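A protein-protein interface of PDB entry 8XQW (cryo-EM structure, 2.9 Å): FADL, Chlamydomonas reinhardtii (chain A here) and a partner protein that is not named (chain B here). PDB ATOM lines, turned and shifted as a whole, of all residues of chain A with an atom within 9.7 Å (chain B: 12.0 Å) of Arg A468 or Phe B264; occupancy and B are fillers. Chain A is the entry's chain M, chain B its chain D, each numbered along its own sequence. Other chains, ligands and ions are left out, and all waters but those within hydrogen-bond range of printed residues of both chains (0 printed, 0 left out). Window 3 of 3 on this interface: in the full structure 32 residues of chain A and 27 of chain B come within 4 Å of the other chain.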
ATOM      1  N   ASP A 463       7.441 -13.250  -7.920  1.00  0.00           N
ATOM      2  CA  ASP A 463       7.995 -14.587  -7.975  1.00  0.00           C
ATOM      3  C   ASP A 463       9.487 -14.488  -7.737  1.00  0.00           C
ATOM      4  O   ASP A 463      10.284 -14.589  -8.671  1.00  0.00           O
ATOM      5  CB  ASP A 463       7.718 -15.241  -9.321  1.00  0.00           C
ATOM      6  CG  ASP A 463       6.272 -15.186  -9.700  1.00  0.00           C
ATOM      7  OD1 ASP A 463       5.795 -14.090 -10.043  1.00  0.00           O
ATOM      8  OD2 ASP A 463       5.610 -16.239  -9.665  1.00  0.00           O
ATOM      9  N   GLY A 464       9.866 -14.271  -6.482  1.00  0.00           N
ATOM     10  CA  GLY A 464      11.230 -13.997  -6.114  1.00  0.00           C
ATOM     11  C   GLY A 464      11.770 -12.685  -6.620  1.00  0.00           C
ATOM     12  O   GLY A 464      12.978 -12.460  -6.519  1.00  0.00           O
ATOM     13  N   LEU A 465      10.918 -11.807  -7.139  1.00  0.00           N
ATOM     14  CA  LEU A 465      11.356 -10.647  -7.903  1.00  0.00           C
ATOM     15  C   LEU A 465      12.351 -11.077  -8.970  1.00  0.00           C
ATOM     16  O   LEU A 465      13.429 -10.509  -9.108  1.00  0.00           O
ATOM     17  CB  LEU A 465      11.959  -9.577  -7.002  1.00  0.00           C
ATOM     18  CG  LEU A 465      11.028  -8.748  -6.142  1.00  0.00           C
ATOM     19  CD1 LEU A 465      11.840  -8.014  -5.125  1.00  0.00           C
ATOM     20  CD2 LEU A 465      10.276  -7.783  -6.984  1.00  0.00           C
ATOM     21  N   ASP A 466      11.978 -12.098  -9.727  1.00  0.00           N
ATOM     22  CA  ASP A 466      12.901 -12.795 -10.611  1.00  0.00           C
ATOM     23  C   ASP A 466      12.374 -12.728 -12.032  1.00  0.00           C
ATOM     24  O   ASP A 466      11.415 -13.420 -12.370  1.00  0.00           O
ATOM     25  CB  ASP A 466      13.069 -14.239 -10.169  1.00  0.00           C
ATOM     26  CG  ASP A 466      14.412 -14.787 -10.512  1.00  0.00           C
ATOM     27  OD1 ASP A 466      14.907 -14.491 -11.608  1.00  0.00           O
ATOM     28  OD2 ASP A 466      14.980 -15.516  -9.682  1.00  0.00           O
ATOM     29  N   LEU A 467      13.010 -11.915 -12.866  1.00  0.00           N
ATOM     30  CA  LEU A 467      12.597 -11.796 -14.253  1.00  0.00           C
ATOM     31  C   LEU A 467      12.927 -13.026 -15.068  1.00  0.00           C
ATOM     32  O   LEU A 467      12.763 -12.996 -16.287  1.00  0.00           O
ATOM     33  CB  LEU A 467      13.262 -10.594 -14.896  1.00  0.00           C
ATOM     34  CG  LEU A 467      12.641  -9.241 -14.641  1.00  0.00           C
ATOM     35  CD1 LEU A 467      13.468  -8.221 -15.334  1.00  0.00           C
ATOM     36  CD2 LEU A 467      11.252  -9.235 -15.167  1.00  0.00           C
ATOM     37  N   ARG A 468      13.412 -14.092 -14.452  1.00  0.00           N
ATOM     38  CA  ARG A 468      13.769 -15.277 -15.214  1.00  0.00           C
ATOM     39  C   ARG A 468      12.655 -16.298 -15.267  1.00  0.00           C
ATOM     40  O   ARG A 468      12.871 -17.395 -15.775  1.00  0.00           O
ATOM     41  CB  ARG A 468      15.029 -15.916 -14.641  1.00  0.00           C
ATOM     42  CG  ARG A 468      16.300 -15.391 -15.272  1.00  0.00           C
ATOM     43  CD  ARG A 468      17.535 -15.887 -14.563  1.00  0.00           C
ATOM     44  NE  ARG A 468      17.545 -15.496 -13.164  1.00  0.00           N
ATOM     45  CZ  ARG A 468      18.260 -16.107 -12.232  1.00  0.00           C
ATOM     46  NH1 ARG A 468      19.020 -17.136 -12.555  1.00  0.00           N
ATOM     47  NH2 ARG A 468      18.210 -15.695 -10.977  1.00  0.00           N
ATOM     48  N   HIS A 469      11.475 -15.968 -14.761  1.00  0.00           N
ATOM     49  CA  HIS A 469      10.317 -16.838 -14.860  1.00  0.00           C
ATOM     50  C   HIS A 469       9.444 -16.516 -16.050  1.00  0.00           C
ATOM     51  O   HIS A 469       8.591 -17.327 -16.406  1.00  0.00           O
ATOM     52  CB  HIS A 469       9.460 -16.736 -13.606  1.00  0.00           C
ATOM     53  CG  HIS A 469      10.078 -17.349 -12.399  1.00  0.00           C
ATOM     54  ND1 HIS A 469      10.000 -16.771 -11.155  1.00  0.00           N
ATOM     55  CD2 HIS A 469      10.782 -18.491 -12.240  1.00  0.00           C
ATOM     56  CE1 HIS A 469      10.632 -17.531 -10.280  1.00  0.00           C
ATOM     57  NE2 HIS A 469      11.116 -18.580 -10.913  1.00  0.00           N
ATOM     58  N   PHE A 470       9.625 -15.369 -16.663  1.00  0.00           N
ATOM     59  CA  PHE A 470       8.709 -14.855 -17.658  1.00  0.00           C
ATOM     60  C   PHE A 470       9.334 -14.935 -19.039  1.00  0.00           C
ATOM     61  O   PHE A 470      10.508 -15.246 -19.207  1.00  0.00           O
ATOM     62  CB  PHE A 470       8.318 -13.420 -17.312  1.00  0.00           C
ATOM     63  CG  PHE A 470       7.741 -13.271 -15.948  1.00  0.00           C
ATOM     64  CD1 PHE A 470       8.544 -13.048 -14.863  1.00  0.00           C
ATOM     65  CD2 PHE A 470       6.390 -13.361 -15.750  1.00  0.00           C
ATOM     66  CE1 PHE A 470       8.017 -12.921 -13.616  1.00  0.00           C
ATOM     67  CE2 PHE A 470       5.862 -13.233 -14.501  1.00  0.00           C
ATOM     68  CZ  PHE A 470       6.677 -13.011 -13.435  1.00  0.00           C
ATOM     69  N   HIS A 471       8.526 -14.661 -20.019  1.00  0.00           N
ATOM     70  CA  HIS A 471       8.938 -14.574 -21.405  1.00  0.00           C
ATOM     71  C   HIS A 471       9.653 -13.251 -21.627  1.00  0.00           C
ATOM     72  O   HIS A 471       9.149 -12.212 -21.204  1.00  0.00           O
ATOM     73  CB  HIS A 471       7.700 -14.669 -22.276  1.00  0.00           C
ATOM     74  CG  HIS A 471       7.978 -14.809 -23.732  1.00  0.00           C
ATOM     75  ND1 HIS A 471       8.339 -13.745 -24.523  1.00  0.00           N
ATOM     76  CD2 HIS A 471       7.903 -15.878 -24.552  1.00  0.00           C
ATOM     77  CE1 HIS A 471       8.502 -14.158 -25.763  1.00  0.00           C
ATOM     78  NE2 HIS A 471       8.246 -15.449 -25.806  1.00  0.00           N
ATOM     79  N   PRO A 472      10.816 -13.242 -22.280  1.00  0.00           N
ATOM     80  CA  PRO A 472      11.567 -11.988 -22.418  1.00  0.00           C
ATOM     81  C   PRO A 472      10.794 -10.848 -23.040  1.00  0.00           C
ATOM     82  O   PRO A 472      10.927  -9.705 -22.594  1.00  0.00           O
ATOM     83  CB  PRO A 472      12.745 -12.406 -23.289  1.00  0.00           C
ATOM     84  CG  PRO A 472      12.954 -13.789 -22.934  1.00  0.00           C
ATOM     85  CD  PRO A 472      11.600 -14.380 -22.763  1.00  0.00           C
ATOM     86  N   SER A 474       8.209  -9.654 -22.565  1.00  0.00           N
ATOM     87  CA  SER A 474       7.314  -8.975 -21.654  1.00  0.00           C
ATOM     88  C   SER A 474       8.009  -8.281 -20.502  1.00  0.00           C
ATOM     89  O   SER A 474       7.318  -7.774 -19.618  1.00  0.00           O
ATOM     90  CB  SER A 474       6.303  -9.960 -21.079  1.00  0.00           C
ATOM     91  OG  SER A 474       6.942 -10.834 -20.191  1.00  0.00           O
ATOM     92  N   TYR A 475       9.341  -8.233 -20.478  1.00  0.00           N
ATOM     93  CA  TYR A 475      10.031  -7.724 -19.299  1.00  0.00           C
ATOM     94  C   TYR A 475       9.534  -6.342 -18.922  1.00  0.00           C
ATOM     95  O   TYR A 475       9.110  -6.117 -17.788  1.00  0.00           O
ATOM     96  CB  TYR A 475      11.530  -7.705 -19.531  1.00  0.00           C
ATOM     97  CG  TYR A 475      12.151  -9.050 -19.357  1.00  0.00           C
ATOM     98  CD1 TYR A 475      11.409 -10.107 -18.906  1.00  0.00           C
ATOM     99  CD2 TYR A 475      13.474  -9.263 -19.636  1.00  0.00           C
ATOM    100  CE1 TYR A 475      11.955 -11.325 -18.749  1.00  0.00           C
ATOM    101  CE2 TYR A 475      14.030 -10.484 -19.476  1.00  0.00           C
ATOM    102  CZ  TYR A 475      13.266 -11.513 -19.031  1.00  0.00           C
ATOM    103  OH  TYR A 475      13.814 -12.755 -18.865  1.00  0.00           O
ATOM    104  N   VAL A 478       6.227  -6.392 -17.200  1.00  0.00           N
ATOM    105  CA  VAL A 478       6.208  -6.965 -15.864  1.00  0.00           C
ATOM    106  C   VAL A 478       6.852  -6.016 -14.873  1.00  0.00           C
ATOM    107  O   VAL A 478       6.314  -5.766 -13.793  1.00  0.00           O
ATOM    108  CB  VAL A 478       6.899  -8.333 -15.861  1.00  0.00           C
ATOM    109  CG1 VAL A 478       7.236  -8.713 -14.479  1.00  0.00           C
ATOM    110  CG2 VAL A 478       5.986  -9.349 -16.454  1.00  0.00           C
ATOM    111  N   LEU A 479       8.005  -5.455 -15.233  1.00  0.00           N
ATOM    112  CA  LEU A 479       8.673  -4.503 -14.359  1.00  0.00           C
ATOM    113  C   LEU A 479       7.750  -3.360 -13.987  1.00  0.00           C
ATOM    114  O   LEU A 479       7.601  -3.034 -12.809  1.00  0.00           O
ATOM    115  CB  LEU A 479       9.930  -3.966 -15.030  1.00  0.00           C
ATOM    116  CG  LEU A 479      11.189  -4.801 -14.895  1.00  0.00           C
ATOM    117  CD1 LEU A 479      12.235  -4.299 -15.846  1.00  0.00           C
ATOM    118  CD2 LEU A 479      11.693  -4.731 -13.495  1.00  0.00           C
ATOM    119  N   TRP A 482       5.406  -4.226 -11.286  1.00  0.00           N
ATOM    120  CA  TRP A 482       5.943  -4.253  -9.935  1.00  0.00           C
ATOM    121  C   TRP A 482       6.221  -2.870  -9.398  1.00  0.00           C
ATOM    122  O   TRP A 482       6.432  -2.724  -8.197  1.00  0.00           O
ATOM    123  CB  TRP A 482       7.244  -5.037  -9.875  1.00  0.00           C
ATOM    124  CG  TRP A 482       7.100  -6.483  -9.928  1.00  0.00           C
ATOM    125  CD1 TRP A 482       6.066  -7.215  -9.473  1.00  0.00           C
ATOM    126  CD2 TRP A 482       8.040  -7.403 -10.464  1.00  0.00           C
ATOM    127  NE1 TRP A 482       6.292  -8.540  -9.695  1.00  0.00           N
ATOM    128  CE2 TRP A 482       7.509  -8.680 -10.301  1.00  0.00           C
ATOM    129  CE3 TRP A 482       9.287  -7.266 -11.067  1.00  0.00           C
ATOM    130  CZ2 TRP A 482       8.169  -9.810 -10.723  1.00  0.00           C
ATOM    131  CZ3 TRP A 482       9.940  -8.388 -11.477  1.00  0.00           C
ATOM    132  CH2 TRP A 482       9.382  -9.643 -11.307  1.00  0.00           C
ATOM    133  N   TYR B  52      -5.243 -24.635 -25.157  1.00  0.00           N
ATOM    134  CA  TYR B  52      -3.968 -24.666 -24.448  1.00  0.00           C
ATOM    135  C   TYR B  52      -3.471 -26.087 -24.220  1.00  0.00           C
ATOM    136  O   TYR B  52      -2.279 -26.367 -24.379  1.00  0.00           O
ATOM    137  CB  TYR B  52      -4.096 -23.945 -23.111  1.00  0.00           C
ATOM    138  CG  TYR B  52      -2.896 -24.119 -22.219  1.00  0.00           C
ATOM    139  CD1 TYR B  52      -1.787 -23.307 -22.359  1.00  0.00           C
ATOM    140  CD2 TYR B  52      -2.869 -25.096 -21.240  1.00  0.00           C
ATOM    141  CE1 TYR B  52      -0.697 -23.457 -21.554  1.00  0.00           C
ATOM    142  CE2 TYR B  52      -1.781 -25.254 -20.430  1.00  0.00           C
ATOM    143  CZ  TYR B  52      -0.697 -24.431 -20.591  1.00  0.00           C
ATOM    144  OH  TYR B  52       0.398 -24.582 -19.782  1.00  0.00           O
ATOM    145  N   PHE B 264      12.704 -22.441 -13.808  1.00  0.00           N
ATOM    146  CA  PHE B 264      12.626 -21.180 -14.528  1.00  0.00           C
ATOM    147  C   PHE B 264      11.841 -21.331 -15.823  1.00  0.00           C
ATOM    148  O   PHE B 264      11.515 -22.441 -16.235  1.00  0.00           O
ATOM    149  CB  PHE B 264      14.022 -20.650 -14.821  1.00  0.00           C
ATOM    150  CG  PHE B 264      14.714 -20.091 -13.618  1.00  0.00           C
ATOM    151  CD1 PHE B 264      13.987 -19.694 -12.511  1.00  0.00           C
ATOM    152  CD2 PHE B 264      16.087 -19.961 -13.590  1.00  0.00           C
ATOM    153  CE1 PHE B 264      14.619 -19.179 -11.403  1.00  0.00           C
ATOM    154  CE2 PHE B 264      16.720 -19.448 -12.484  1.00  0.00           C
ATOM    155  CZ  PHE B 264      15.983 -19.057 -11.390  1.00  0.00           C
ATOM    156  N   GLY B 265      11.548 -20.201 -16.460  1.00  0.00           N
ATOM    157  CA  GLY B 265      10.738 -20.201 -17.666  1.00  0.00           C
ATOM    158  C   GLY B 265       9.388 -20.845 -17.471  1.00  0.00           C
ATOM    159  O   GLY B 265       8.890 -21.516 -18.380  1.00  0.00           O
ATOM    160  N   THR B 266       8.782 -20.665 -16.304  1.00  0.00           N
ATOM    161  CA  THR B 266       7.537 -21.343 -15.990  1.00  0.00           C
ATOM    162  C   THR B 266       6.325 -20.704 -16.644  1.00  0.00           C
ATOM    163  O   THR B 266       5.361 -21.409 -16.939  1.00  0.00           O
ATOM    164  CB  THR B 266       7.330 -21.398 -14.478  1.00  0.00           C
ATOM    165  OG1 THR B 266       6.649 -20.224 -14.043  1.00  0.00           O
ATOM    166  CG2 THR B 266       8.649 -21.476 -13.771  1.00  0.00           C
ATOM    167  N   TYR B 267       6.345 -19.398 -16.885  1.00  0.00           N
ATOM    168  CA  TYR B 267       5.252 -18.743 -17.583  1.00  0.00           C
ATOM    169  C   TYR B 267       5.588 -18.465 -19.032  1.00  0.00           C
ATOM    170  O   TYR B 267       4.871 -17.709 -19.683  1.00  0.00           O
ATOM    171  CB  TYR B 267       4.872 -17.430 -16.909  1.00  0.00           C
ATOM    172  CG  TYR B 267       4.589 -17.567 -15.452  1.00  0.00           C
ATOM    173  CD1 TYR B 267       3.458 -18.210 -15.005  1.00  0.00           C
ATOM    174  CD2 TYR B 267       5.457 -17.055 -14.523  1.00  0.00           C
ATOM    175  CE1 TYR B 267       3.209 -18.334 -13.676  1.00  0.00           C
ATOM    176  CE2 TYR B 267       5.218 -17.176 -13.202  1.00  0.00           C
ATOM    177  CZ  TYR B 267       4.096 -17.814 -12.779  1.00  0.00           C
ATOM    178  OH  TYR B 267       3.863 -17.927 -11.438  1.00  0.00           O
ATOM    179  N   TYR B 268       6.672 -19.037 -19.546  1.00  0.00           N
ATOM    180  CA  TYR B 268       7.058 -18.780 -20.923  1.00  0.00           C
ATOM    181  C   TYR B 268       5.967 -19.218 -21.884  1.00  0.00           C
ATOM    182  O   TYR B 268       5.480 -18.428 -22.703  1.00  0.00           O
ATOM    183  CB  TYR B 268       8.366 -19.502 -21.216  1.00  0.00           C
ATOM    184  CG  TYR B 268       8.998 -19.150 -22.529  1.00  0.00           C
ATOM    185  CD1 TYR B 268       8.512 -19.668 -23.711  1.00  0.00           C
ATOM    186  CD2 TYR B 268      10.091 -18.320 -22.586  1.00  0.00           C
ATOM    187  CE1 TYR B 268       9.082 -19.358 -24.905  1.00  0.00           C
ATOM    188  CE2 TYR B 268      10.669 -18.003 -23.781  1.00  0.00           C
ATOM    189  CZ  TYR B 268      10.159 -18.526 -24.938  1.00  0.00           C
ATOM    190  OH  TYR B 268      10.735 -18.216 -26.140  1.00  0.00           O
ATOM    191  N   PHE B 269       5.557 -20.477 -21.787  1.00  0.00           N
ATOM    192  CA  PHE B 269       4.594 -21.010 -22.736  1.00  0.00           C
ATOM    193  C   PHE B 269       3.232 -20.354 -22.581  1.00  0.00           C
ATOM    194  O   PHE B 269       2.559 -20.068 -23.577  1.00  0.00           O
ATOM    195  CB  PHE B 269       4.487 -22.515 -22.560  1.00  0.00           C
ATOM    196  CG  PHE B 269       3.612 -23.167 -23.565  1.00  0.00           C
ATOM    197  CD1 PHE B 269       4.001 -23.250 -24.884  1.00  0.00           C
ATOM    198  CD2 PHE B 269       2.392 -23.692 -23.196  1.00  0.00           C
ATOM    199  CE1 PHE B 269       3.192 -23.846 -25.815  1.00  0.00           C
ATOM    200  CE2 PHE B 269       1.580 -24.290 -24.121  1.00  0.00           C
ATOM    201  CZ  PHE B 269       1.979 -24.370 -25.432  1.00  0.00           C
ATOM    202  N   LEU B 270       2.807 -20.111 -21.344  1.00  0.00           N
ATOM    203  CA  LEU B 270       1.524 -19.465 -21.112  1.00  0.00           C
ATOM    204  C   LEU B 270       1.482 -18.084 -21.745  1.00  0.00           C
ATOM    205  O   LEU B 270       0.514 -17.726 -22.417  1.00  0.00           O
ATOM    206  CB  LEU B 270       1.262 -19.371 -19.615  1.00  0.00           C
ATOM    207  CG  LEU B 270      -0.166 -19.384 -19.096  1.00  0.00           C
ATOM    208  CD1 LEU B 270      -0.124 -19.688 -17.640  1.00  0.00           C
ATOM    209  CD2 LEU B 270      -0.805 -18.056 -19.300  1.00  0.00           C
ATOM    210  N   GLN B 271       2.528 -17.291 -21.538  1.00  0.00           N
ATOM    211  CA  GLN B 271       2.540 -15.942 -22.081  1.00  0.00           C
ATOM    212  C   GLN B 271       2.602 -15.960 -23.596  1.00  0.00           C
ATOM    213  O   GLN B 271       1.976 -15.127 -24.257  1.00  0.00           O
ATOM    214  CB  GLN B 271       3.717 -15.165 -21.524  1.00  0.00           C
ATOM    215  CG  GLN B 271       3.594 -14.844 -20.081  1.00  0.00           C
ATOM    216  CD  GLN B 271       4.595 -13.833 -19.653  1.00  0.00           C
ATOM    217  OE1 GLN B 271       4.354 -12.638 -19.714  1.00  0.00           O
ATOM    218  NE2 GLN B 271       5.735 -14.304 -19.216  1.00  0.00           N
ATOM    219  N   ASN B2374      11.732  -5.958 -25.791  1.00  0.00           N
ATOM    220  CA  ASN B2374      11.160  -6.353 -24.511  1.00  0.00           C
ATOM    221  C   ASN B2374       9.785  -5.749 -24.294  1.00  0.00           C
ATOM    222  O   ASN B2374       9.323  -5.673 -23.161  1.00  0.00           O
ATOM    223  CB  ASN B2374      12.072  -5.948 -23.361  1.00  0.00           C
ATOM    224  CG  ASN B2374      13.348  -6.719 -23.335  1.00  0.00           C
ATOM    225  OD1 ASN B2374      13.356  -7.928 -23.162  1.00  0.00           O
ATOM    226  ND2 ASN B2374      14.449  -6.020 -23.490  1.00  0.00           N
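The side-chain carboxylate (OD2) of Asp A463 is in hydrogen-bond range of the side-chain hydroxyl (OH) of Tyr B267 (3.0 Å). O of Arg A468 is in hydrogen-bond range of N of Gly B265, 3.2 Å away. O of His A469 sits at hydrogen-bond distance from N of Thr B266, 3.3 Å away. The backbone carbonyl oxygen (O) of His A469 is in hydrogen-bond range of the backbone NH (N) of Tyr B267, 3.1 Å away. The backbone NH of His A471 lies close to the side-chain amide nitrogen of Gln B271, at 2.9 Å. The backbone carbonyl oxygen (O) of Pro A472 sits close to the side-chain amide oxygen (OD1) of Asn B2374 (3.1 Å). OG of Ser A474 sits at hydrogen-bond distance from OE1 of Gln B271, 3.2 Å away.
O of Asp A463 lies close to ND1 of His A469 (3.3 Å). The guanidinium group of Arg A468 is in salt-bridge range of the side-chain carboxylate of Asp A466 (3.2 Å). The side-chain hydroxyl (OH) of Tyr A475 is in hydrogen-bond range of the backbone carbonyl oxygen (O) of Leu A467. The backbone carbonyl oxygen of His A471 sits at hydrogen-bond distance from the side-chain hydroxyl of Ser A474 (2.8 Å).
Arg A468 touches Phe B264 (NH1 to CE2, 3.3 Å). His A469 touches Phe B264 (CD2 to CD1, 3.4 Å). His A469 touches Gly B265 (O to C, 3.8 Å). CD2 of Tyr B267 touches CE2 of Phe A470 (3.8 Å). Gln B271 touches Phe A470 (NE2 to CB, 3.3 Å). CZ of Tyr B268 touches CD2 of His A471 (3.5 Å). Pro A472 touches Tyr B268 (CD to CE2, 3.9 Å). Asn B2374 touches Ser A474. Asn B2374 touches Tyr A475.
Arg A468 touches just these residues of chain B: Phe B264 (3.3 Å) and Gly B265 (3.2 Å). No residue of chain B comes within 4 Å of Leu A467. His A469 touches four residues of chain B. Of the printed residues of chain B, Phe A470 touches Tyr B267 (3.8 Å) and Gln B271 (3.3 Å). Of chain A, only Arg A468 (3.2 Å) and His A469 (3.8 Å) come within 4 Å of Gly B265. Printed residues of chain A within 4 Å of Tyr B267: Asp A463, His A469 and Phe A470. Printed residues of chain A within 4 Å of Thr B266: His A469. Of the printed residues of chain A, Asn B2374 touches Pro A472, Ser A474 and Tyr A475. Of the printed residues of chain A, Gln B271 touches Phe A470 (3.3 Å), His A471 (2.9 Å) and Ser A474 (3.2 Å). Of the printed residues of chain B, Pro A472 touches Tyr B268 (3.9 Å) and Asn B2374 (3.1 Å). Leu B270 touches none of the printed residues of chain A.
Printed residues of chain B that touch a printed residue of chain A: Phe B264, Gly B265, Thr B266, Tyr B267, Tyr B268, Gln B271 and Asn B2374. Of the 15 printed residues of chain A, 8 touch a printed residue of chain B. Printed residues of chain A that touch a printed residue of chain B: Asp A463, Arg A468, His A469, Phe A470, His A471, Pro A472, Ser A474 and Tyr A475. Among the printed residues, 16 pairs touch across the chains. Among the printed residues, no Asp or Glu carboxylate lies within 4 Å of a Lys or Arg side-chain nitrogen of the other chain.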
